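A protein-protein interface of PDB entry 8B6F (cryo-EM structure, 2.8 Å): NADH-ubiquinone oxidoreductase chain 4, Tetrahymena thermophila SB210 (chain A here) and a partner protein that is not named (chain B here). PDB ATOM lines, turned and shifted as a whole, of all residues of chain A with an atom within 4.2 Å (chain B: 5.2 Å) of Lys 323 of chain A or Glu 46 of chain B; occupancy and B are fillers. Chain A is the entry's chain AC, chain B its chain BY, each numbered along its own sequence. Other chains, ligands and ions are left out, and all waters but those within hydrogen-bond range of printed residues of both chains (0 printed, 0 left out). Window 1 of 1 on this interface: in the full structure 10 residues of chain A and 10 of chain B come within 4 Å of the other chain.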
ATOM      1  N   HIS A 263      -5.304   3.007  27.592  1.00  0.00           N
ATOM      2  CA  HIS A 263      -5.276   4.413  27.963  1.00  0.00           C
ATOM      3  C   HIS A 263      -5.085   5.317  26.756  1.00  0.00           C
ATOM      4  O   HIS A 263      -4.951   6.534  26.928  1.00  0.00           O
ATOM      5  CB  HIS A 263      -4.179   4.691  29.003  1.00  0.00           C
ATOM      6  CG  HIS A 263      -2.811   4.254  28.583  1.00  0.00           C
ATOM      7  ND1 HIS A 263      -2.096   4.897  27.596  1.00  0.00           N
ATOM      8  CD2 HIS A 263      -2.022   3.249  29.026  1.00  0.00           C
ATOM      9  CE1 HIS A 263      -0.927   4.302  27.444  1.00  0.00           C
ATOM     10  NE2 HIS A 263      -0.856   3.299  28.299  1.00  0.00           N
ATOM     11  N   ASP A 319       4.716   2.049  32.779  1.00  0.00           N
ATOM     12  CA  ASP A 319       4.622   2.632  31.446  1.00  0.00           C
ATOM     13  C   ASP A 319       4.370   4.132  31.518  1.00  0.00           C
ATOM     14  O   ASP A 319       5.044   4.919  30.844  1.00  0.00           O
ATOM     15  CB  ASP A 319       3.516   1.919  30.664  1.00  0.00           C
ATOM     16  CG  ASP A 319       3.252   2.546  29.310  1.00  0.00           C
ATOM     17  OD1 ASP A 319       2.822   3.717  29.262  1.00  0.00           O
ATOM     18  OD2 ASP A 319       3.472   1.865  28.288  1.00  0.00           O
ATOM     19  N   SER A 320       3.398   4.549  32.329  1.00  0.00           N
ATOM     20  CA  SER A 320       3.098   5.973  32.448  1.00  0.00           C
ATOM     21  C   SER A 320       4.286   6.746  33.005  1.00  0.00           C
ATOM     22  O   SER A 320       4.621   7.826  32.510  1.00  0.00           O
ATOM     23  CB  SER A 320       1.865   6.174  33.327  1.00  0.00           C
ATOM     24  OG  SER A 320       2.041   5.567  34.594  1.00  0.00           O
ATOM     25  N   SER A 321       4.939   6.206  34.036  1.00  0.00           N
ATOM     26  CA  SER A 321       6.073   6.895  34.644  1.00  0.00           C
ATOM     27  C   SER A 321       7.217   7.068  33.655  1.00  0.00           C
ATOM     28  O   SER A 321       7.833   8.138  33.586  1.00  0.00           O
ATOM     29  CB  SER A 321       6.550   6.121  35.872  1.00  0.00           C
ATOM     30  OG  SER A 321       5.509   5.987  36.822  1.00  0.00           O
ATOM     31  N   LEU A 322       7.512   6.030  32.875  1.00  0.00           N
ATOM     32  CA  LEU A 322       8.593   6.121  31.901  1.00  0.00           C
ATOM     33  C   LEU A 322       8.262   7.110  30.791  1.00  0.00           C
ATOM     34  O   LEU A 322       9.153   7.805  30.289  1.00  0.00           O
ATOM     35  CB  LEU A 322       8.891   4.739  31.314  1.00  0.00           C
ATOM     36  CG  LEU A 322       9.482   3.692  32.264  1.00  0.00           C
ATOM     37  CD1 LEU A 322       9.663   2.362  31.552  1.00  0.00           C
ATOM     38  CD2 LEU A 322      10.807   4.164  32.839  1.00  0.00           C
ATOM     39  N   LYS A 323       6.994   7.186  30.389  1.00  0.00           N
ATOM     40  CA  LYS A 323       6.605   8.093  29.315  1.00  0.00           C
ATOM     41  C   LYS A 323       6.474   9.540  29.771  1.00  0.00           C
ATOM     42  O   LYS A 323       6.432  10.436  28.922  1.00  0.00           O
ATOM     43  CB  LYS A 323       5.281   7.635  28.699  1.00  0.00           C
ATOM     44  CG  LYS A 323       5.372   6.315  27.955  1.00  0.00           C
ATOM     45  CD  LYS A 323       4.014   5.859  27.457  1.00  0.00           C
ATOM     46  CE  LYS A 323       4.109   4.488  26.815  1.00  0.00           C
ATOM     47  NZ  LYS A 323       2.770   3.888  26.569  1.00  0.00           N
ATOM     48  N   MET A 324       6.404   9.793  31.079  1.00  0.00           N
ATOM     49  CA  MET A 324       6.255  11.164  31.558  1.00  0.00           C
ATOM     50  C   MET A 324       7.325  12.087  30.986  1.00  0.00           C
ATOM     51  O   MET A 324       7.044  13.243  30.653  1.00  0.00           O
ATOM     52  CB  MET A 324       6.302  11.196  33.084  1.00  0.00           C
ATOM     53  CG  MET A 324       4.990  10.838  33.736  1.00  0.00           C
ATOM     54  SD  MET A 324       5.098  10.844  35.527  1.00  0.00           S
ATOM     55  CE  MET A 324       3.504  10.159  35.925  1.00  0.00           C
ATOM     56  N   TRP A 325       8.560  11.598  30.868  1.00  0.00           N
ATOM     57  CA  TRP A 325       9.660  12.481  30.488  1.00  0.00           C
ATOM     58  C   TRP A 325       9.464  13.050  29.088  1.00  0.00           C
ATOM     59  O   TRP A 325       9.766  14.223  28.841  1.00  0.00           O
ATOM     60  CB  TRP A 325      10.988  11.731  30.571  1.00  0.00           C
ATOM     61  CG  TRP A 325      12.153  12.512  30.036  1.00  0.00           C
ATOM     62  CD1 TRP A 325      12.524  12.636  28.729  1.00  0.00           C
ATOM     63  CD2 TRP A 325      13.099  13.274  30.795  1.00  0.00           C
ATOM     64  NE1 TRP A 325      13.641  13.427  28.628  1.00  0.00           N
ATOM     65  CE2 TRP A 325      14.015  13.830  29.882  1.00  0.00           C
ATOM     66  CE3 TRP A 325      13.262  13.536  32.159  1.00  0.00           C
ATOM     67  CZ2 TRP A 325      15.076  14.637  30.287  1.00  0.00           C
ATOM     68  CZ3 TRP A 325      14.316  14.336  32.560  1.00  0.00           C
ATOM     69  CH2 TRP A 325      15.211  14.877  31.626  1.00  0.00           C
ATOM     70  N   GLY A 326       8.971  12.239  28.159  1.00  0.00           N
ATOM     71  CA  GLY A 326       8.947  12.610  26.762  1.00  0.00           C
ATOM     72  C   GLY A 326       7.796  13.485  26.326  1.00  0.00           C
ATOM     73  O   GLY A 326       7.577  13.633  25.122  1.00  0.00           O
ATOM     74  N   GLN A 327       7.045  14.065  27.258  1.00  0.00           N
ATOM     75  CA  GLN A 327       5.893  14.900  26.938  1.00  0.00           C
ATOM     76  C   GLN A 327       6.246  16.365  27.153  1.00  0.00           C
ATOM     77  O   GLN A 327       6.519  16.780  28.283  1.00  0.00           O
ATOM     78  CB  GLN A 327       4.687  14.515  27.797  1.00  0.00           C
ATOM     79  CG  GLN A 327       3.723  13.561  27.119  1.00  0.00           C
ATOM     80  CD  GLN A 327       4.395  12.295  26.642  1.00  0.00           C
ATOM     81  OE1 GLN A 327       5.468  11.933  27.118  1.00  0.00           O
ATOM     82  NE2 GLN A 327       3.771  11.618  25.686  1.00  0.00           N
ATOM     83  N   TYR A 336      -0.813  11.557  31.759  1.00  0.00           N
ATOM     84  CA  TYR A 336       0.016  10.420  32.148  1.00  0.00           C
ATOM     85  C   TYR A 336       0.104  10.306  33.665  1.00  0.00           C
ATOM     86  O   TYR A 336       0.092   9.198  34.210  1.00  0.00           O
ATOM     87  CB  TYR A 336       1.405  10.538  31.524  1.00  0.00           C
ATOM     88  CG  TYR A 336       1.441  10.084  30.085  1.00  0.00           C
ATOM     89  CD1 TYR A 336       1.272   8.745  29.756  1.00  0.00           C
ATOM     90  CD2 TYR A 336       1.642  10.989  29.055  1.00  0.00           C
ATOM     91  CE1 TYR A 336       1.299   8.323  28.443  1.00  0.00           C
ATOM     92  CE2 TYR A 336       1.672  10.577  27.740  1.00  0.00           C
ATOM     93  CZ  TYR A 336       1.501   9.244  27.441  1.00  0.00           C
ATOM     94  OH  TYR A 336       1.531   8.829  26.130  1.00  0.00           O
ATOM     95  N   SER B  41      10.316   4.047  25.477  1.00  0.00           N
ATOM     96  CA  SER B  41       9.083   4.369  26.185  1.00  0.00           C
ATOM     97  C   SER B  41       8.074   5.083  25.291  1.00  0.00           C
ATOM     98  O   SER B  41       6.930   4.639  25.158  1.00  0.00           O
ATOM     99  CB  SER B  41       9.399   5.224  27.412  1.00  0.00           C
ATOM    100  OG  SER B  41       8.210   5.518  28.116  1.00  0.00           O
ATOM    101  N   ILE B  42       8.480   6.191  24.677  1.00  0.00           N
ATOM    102  CA  ILE B  42       7.548   6.974  23.870  1.00  0.00           C
ATOM    103  C   ILE B  42       7.244   6.254  22.562  1.00  0.00           C
ATOM    104  O   ILE B  42       6.094   5.903  22.280  1.00  0.00           O
ATOM    105  CB  ILE B  42       8.105   8.388  23.625  1.00  0.00           C
ATOM    106  CG1 ILE B  42       8.228   9.154  24.945  1.00  0.00           C
ATOM    107  CG2 ILE B  42       7.237   9.149  22.639  1.00  0.00           C
ATOM    108  CD1 ILE B  42       6.906   9.466  25.620  1.00  0.00           C
ATOM    109  N   PHE B  43       8.267   6.012  21.747  1.00  0.00           N
ATOM    110  CA  PHE B  43       8.020   5.465  20.418  1.00  0.00           C
ATOM    111  C   PHE B  43       7.660   3.986  20.486  1.00  0.00           C
ATOM    112  O   PHE B  43       6.555   3.587  20.104  1.00  0.00           O
ATOM    113  CB  PHE B  43       9.235   5.702  19.524  1.00  0.00           C
ATOM    114  CG  PHE B  43       9.444   7.146  19.181  1.00  0.00           C
ATOM    115  CD1 PHE B  43       8.677   7.752  18.202  1.00  0.00           C
ATOM    116  CD2 PHE B  43      10.393   7.901  19.845  1.00  0.00           C
ATOM    117  CE1 PHE B  43       8.857   9.082  17.886  1.00  0.00           C
ATOM    118  CE2 PHE B  43      10.578   9.231  19.533  1.00  0.00           C
ATOM    119  CZ  PHE B  43       9.809   9.822  18.552  1.00  0.00           C
ATOM    120  N   PHE B  44       8.569   3.151  20.983  1.00  0.00           N
ATOM    121  CA  PHE B  44       8.256   1.728  21.055  1.00  0.00           C
ATOM    122  C   PHE B  44       7.081   1.476  21.989  1.00  0.00           C
ATOM    123  O   PHE B  44       6.217   0.642  21.700  1.00  0.00           O
ATOM    124  CB  PHE B  44       9.472   0.922  21.501  1.00  0.00           C
ATOM    125  CG  PHE B  44       9.240  -0.561  21.483  1.00  0.00           C
ATOM    126  CD1 PHE B  44       9.390  -1.284  20.313  1.00  0.00           C
ATOM    127  CD2 PHE B  44       8.855  -1.228  22.633  1.00  0.00           C
ATOM    128  CE1 PHE B  44       9.170  -2.643  20.291  1.00  0.00           C
ATOM    129  CE2 PHE B  44       8.633  -2.587  22.619  1.00  0.00           C
ATOM    130  CZ  PHE B  44       8.791  -3.297  21.447  1.00  0.00           C
ATOM    131  N   GLY B  45       7.033   2.178  23.113  1.00  0.00           N
ATOM    132  CA  GLY B  45       5.946   2.003  24.051  1.00  0.00           C
ATOM    133  C   GLY B  45       4.646   2.629  23.591  1.00  0.00           C
ATOM    134  O   GLY B  45       3.672   1.916  23.336  1.00  0.00           O
ATOM    135  N   GLU B  46       4.605   3.957  23.479  1.00  0.00           N
ATOM    136  CA  GLU B  46       3.341   4.622  23.177  1.00  0.00           C
ATOM    137  C   GLU B  46       2.929   4.420  21.722  1.00  0.00           C
ATOM    138  O   GLU B  46       1.767   4.111  21.437  1.00  0.00           O
ATOM    139  CB  GLU B  46       3.432   6.112  23.511  1.00  0.00           C
ATOM    140  CG  GLU B  46       2.113   6.858  23.382  1.00  0.00           C
ATOM    141  CD  GLU B  46       1.027   6.297  24.281  1.00  0.00           C
ATOM    142  OE1 GLU B  46       1.361   5.589  25.253  1.00  0.00           O
ATOM    143  OE2 GLU B  46      -0.162   6.562  24.013  1.00  0.00           O
ATOM    144  N   LYS B  47       3.860   4.583  20.782  1.00  0.00           N
ATOM    145  CA  LYS B  47       3.469   4.493  19.378  1.00  0.00           C
ATOM    146  C   LYS B  47       3.223   3.052  18.942  1.00  0.00           C
ATOM    147  O   LYS B  47       2.260   2.787  18.216  1.00  0.00           O
ATOM    148  CB  LYS B  47       4.524   5.153  18.484  1.00  0.00           C
ATOM    149  CG  LYS B  47       4.470   6.677  18.482  1.00  0.00           C
ATOM    150  CD  LYS B  47       3.214   7.203  17.801  1.00  0.00           C
ATOM    151  CE  LYS B  47       3.188   8.721  17.798  1.00  0.00           C
ATOM    152  NZ  LYS B  47       1.944   9.252  17.181  1.00  0.00           N
ATOM    153  N   PHE B  48       4.075   2.109  19.343  1.00  0.00           N
ATOM    154  CA  PHE B  48       3.895   0.729  18.896  1.00  0.00           C
ATOM    155  C   PHE B  48       3.032  -0.087  19.857  1.00  0.00           C
ATOM    156  O   PHE B  48       1.975  -0.593  19.471  1.00  0.00           O
ATOM    157  CB  PHE B  48       5.253   0.045  18.709  1.00  0.00           C
ATOM    158  CG  PHE B  48       5.166  -1.455  18.657  1.00  0.00           C
ATOM    159  CD1 PHE B  48       4.585  -2.092  17.575  1.00  0.00           C
ATOM    160  CD2 PHE B  48       5.672  -2.227  19.687  1.00  0.00           C
ATOM    161  CE1 PHE B  48       4.504  -3.472  17.525  1.00  0.00           C
ATOM    162  CE2 PHE B  48       5.595  -3.607  19.642  1.00  0.00           C
ATOM    163  CZ  PHE B  48       5.010  -4.229  18.561  1.00  0.00           C
ATOM    164  N   MET B  49       3.466  -0.224  21.111  1.00  0.00           N
ATOM    165  CA  MET B  49       2.768  -1.123  22.024  1.00  0.00           C
ATOM    166  C   MET B  49       1.343  -0.657  22.298  1.00  0.00           C
ATOM    167  O   MET B  49       0.421  -1.475  22.374  1.00  0.00           O
ATOM    168  CB  MET B  49       3.545  -1.258  23.334  1.00  0.00           C
ATOM    169  CG  MET B  49       4.838  -2.044  23.202  1.00  0.00           C
ATOM    170  SD  MET B  49       5.693  -2.288  24.771  1.00  0.00           S
ATOM    171  CE  MET B  49       4.524  -3.316  25.654  1.00  0.00           C
ATOM    172  N   ILE B  50       1.141   0.651  22.449  1.00  0.00           N
ATOM    173  CA  ILE B  50      -0.174   1.185  22.789  1.00  0.00           C
ATOM    174  C   ILE B  50      -0.960   1.511  21.530  1.00  0.00           C
ATOM    175  O   ILE B  50      -2.042   0.961  21.299  1.00  0.00           O
ATOM    176  CB  ILE B  50      -0.047   2.434  23.682  1.00  0.00           C
ATOM    177  CG1 ILE B  50       0.535   2.076  25.051  1.00  0.00           C
ATOM    178  CG2 ILE B  50      -1.401   3.123  23.858  1.00  0.00           C
ATOM    179  CD1 ILE B  50      -0.286   1.099  25.850  1.00  0.00           C
ATOM    180  N   GLU B  51      -0.425   2.416  20.710  1.00  0.00           N
ATOM    181  CA  GLU B  51      -1.200   2.924  19.584  1.00  0.00           C
ATOM    182  C   GLU B  51      -1.319   1.894  18.470  1.00  0.00           C
ATOM    183  O   GLU B  51      -2.393   1.741  17.877  1.00  0.00           O
ATOM    184  CB  GLU B  51      -0.570   4.213  19.056  1.00  0.00           C
ATOM    185  CG  GLU B  51      -1.221   4.739  17.789  1.00  0.00           C
ATOM    186  CD  GLU B  51      -0.657   6.075  17.360  1.00  0.00           C
ATOM    187  OE1 GLU B  51      -0.054   6.764  18.209  1.00  0.00           O
ATOM    188  OE2 GLU B  51      -0.810   6.434  16.175  1.00  0.00           O
ATOM    189  N   TYR B  52      -0.233   1.190  18.151  1.00  0.00           N
ATOM    190  CA  TYR B  52      -0.295   0.265  17.025  1.00  0.00           C
ATOM    191  C   TYR B  52      -0.998  -1.036  17.396  1.00  0.00           C
ATOM    192  O   TYR B  52      -1.941  -1.452  16.716  1.00  0.00           O
ATOM    193  CB  TYR B  52       1.108  -0.033  16.495  1.00  0.00           C
ATOM    194  CG  TYR B  52       1.106  -1.064  15.392  1.00  0.00           C
ATOM    195  CD1 TYR B  52       0.928  -0.692  14.068  1.00  0.00           C
ATOM    196  CD2 TYR B  52       1.272  -2.411  15.676  1.00  0.00           C
ATOM    197  CE1 TYR B  52       0.914  -1.630  13.059  1.00  0.00           C
ATOM    198  CE2 TYR B  52       1.261  -3.358  14.675  1.00  0.00           C
ATOM    199  CZ  TYR B  52       1.082  -2.961  13.368  1.00  0.00           C
ATOM    200  OH  TYR B  52       1.073  -3.901  12.367  1.00  0.00           O
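The side-chain amino group (NZ) of Lys 323 of chain A lies within salt-bridge range of the side-chain carboxylate (OE1) of Glu 46 of chain B (2.6 Å). The side-chain hydroxyl of Tyr 336 of chain A lies close to the side-chain carboxylate of Glu 46 of chain B (3.4 Å). The backbone NH (N) of Lys 323 of chain A lies close to the side-chain hydroxyl (OG) of Ser 41 of chain B, 3.1 Å away. OG of Ser 41 of chain B lies close to O of Leu 322 of chain A, at 3.3 Å.
The side-chain amide oxygen (OE1) of Gln 327 of chain A sits close to the backbone carbonyl oxygen (O) of Lys 323 of chain A (2.5 Å). O of Ile 42 of chain B lies within hydrogen-bond range of N of Lys 47 of chain B, at 3.0 Å. O of Ser 41 of chain B sits at hydrogen-bond distance from N of Glu 46 of chain B (2.9 Å). The side-chain carboxylate (OD1) of Asp 319 of chain A is in salt-bridge range of the side-chain amino group (NZ) of Lys 323 of chain A. The backbone carbonyl oxygen of Glu 46 of chain B sits at hydrogen-bond distance from the backbone NH of Glu 51 of chain B (2.9 Å). The backbone carbonyl oxygen (O) of Gly 45 of chain B lies within hydrogen-bond range of the backbone NH (N) of Ile 50 of chain B (3.0 Å).
His 263 of chain A touches Glu 46 of chain B (CE1 to OE1, 3.4 Å). NE2 of His 263 of chain A touches CD1 of Ile 50 of chain B, at 3.3 Å. CD1 of Ile 42 of chain B touches O of Lys 323 of chain A, 3.5 Å away. Lys 323 of chain A touches Gly 45 of chain B (NZ to C, 3.7 Å). NZ of Lys 323 of chain A touches CG1 of Ile 50 of chain B, 3.3 Å away. Gly 326 of chain A touches Ile 42 of chain B (CA to CD1, 3.9 Å). Gln 327 of chain A touches Ile 42 of chain B (OE1 to CD1, 3.2 Å).
Of the printed residues of chain B, His 263 of chain A touches Glu 46 (3.4 Å) and Ile 50 (3.3 Å). Lys 323 of chain A touches five residues of chain B. Of the printed residues of chain B, Gln 327 of chain A touches Ile 42 (3.2 Å). Glu 46 of chain B touches three residues of chain A. Lys 47 of chain B touches none of the printed residues of chain A. Tyr 52 of chain B touches none of the printed residues of chain A. The nearest printed residue of chain B that does not touch Lys 323 of chain A is Lys 47 of chain B (5.9 Å). The nearest printed residue of chain A that does not touch Glu 46 of chain B is Asp 319 of chain A (4.7 Å). The nearest printed residue of chain A that does not touch Ile 42 of chain B is Tyr 336 of chain A (5.4 Å).
Hydrophobic or aromatic side chains of chain A within 4 Å of the printed part of chain B: His 263, Leu 322 and Tyr 336. Of the 12 printed residues of chain B, 5 touch a printed residue of chain A. Printed residues of chain B that touch a printed residue of chain A: Ser 41, Ile 42, Gly 45, Glu 46 and Ile 50. Hydrophobic or aromatic side chains of chain B within 4 Å of the printed part of chain A: Ile 42 and Ile 50. Along chain B the printed residues that touch a printed residue of chain A span positions 41 to 50. Among the printed residues, 11 pairs touch across the chains. Among the printed residues, Asp or Glu carboxylates within 4 Å of a Lys or Arg side-chain nitrogen of the other chain: Lys 323 of chain A with Glu 46 of chain B (2.6 Å).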
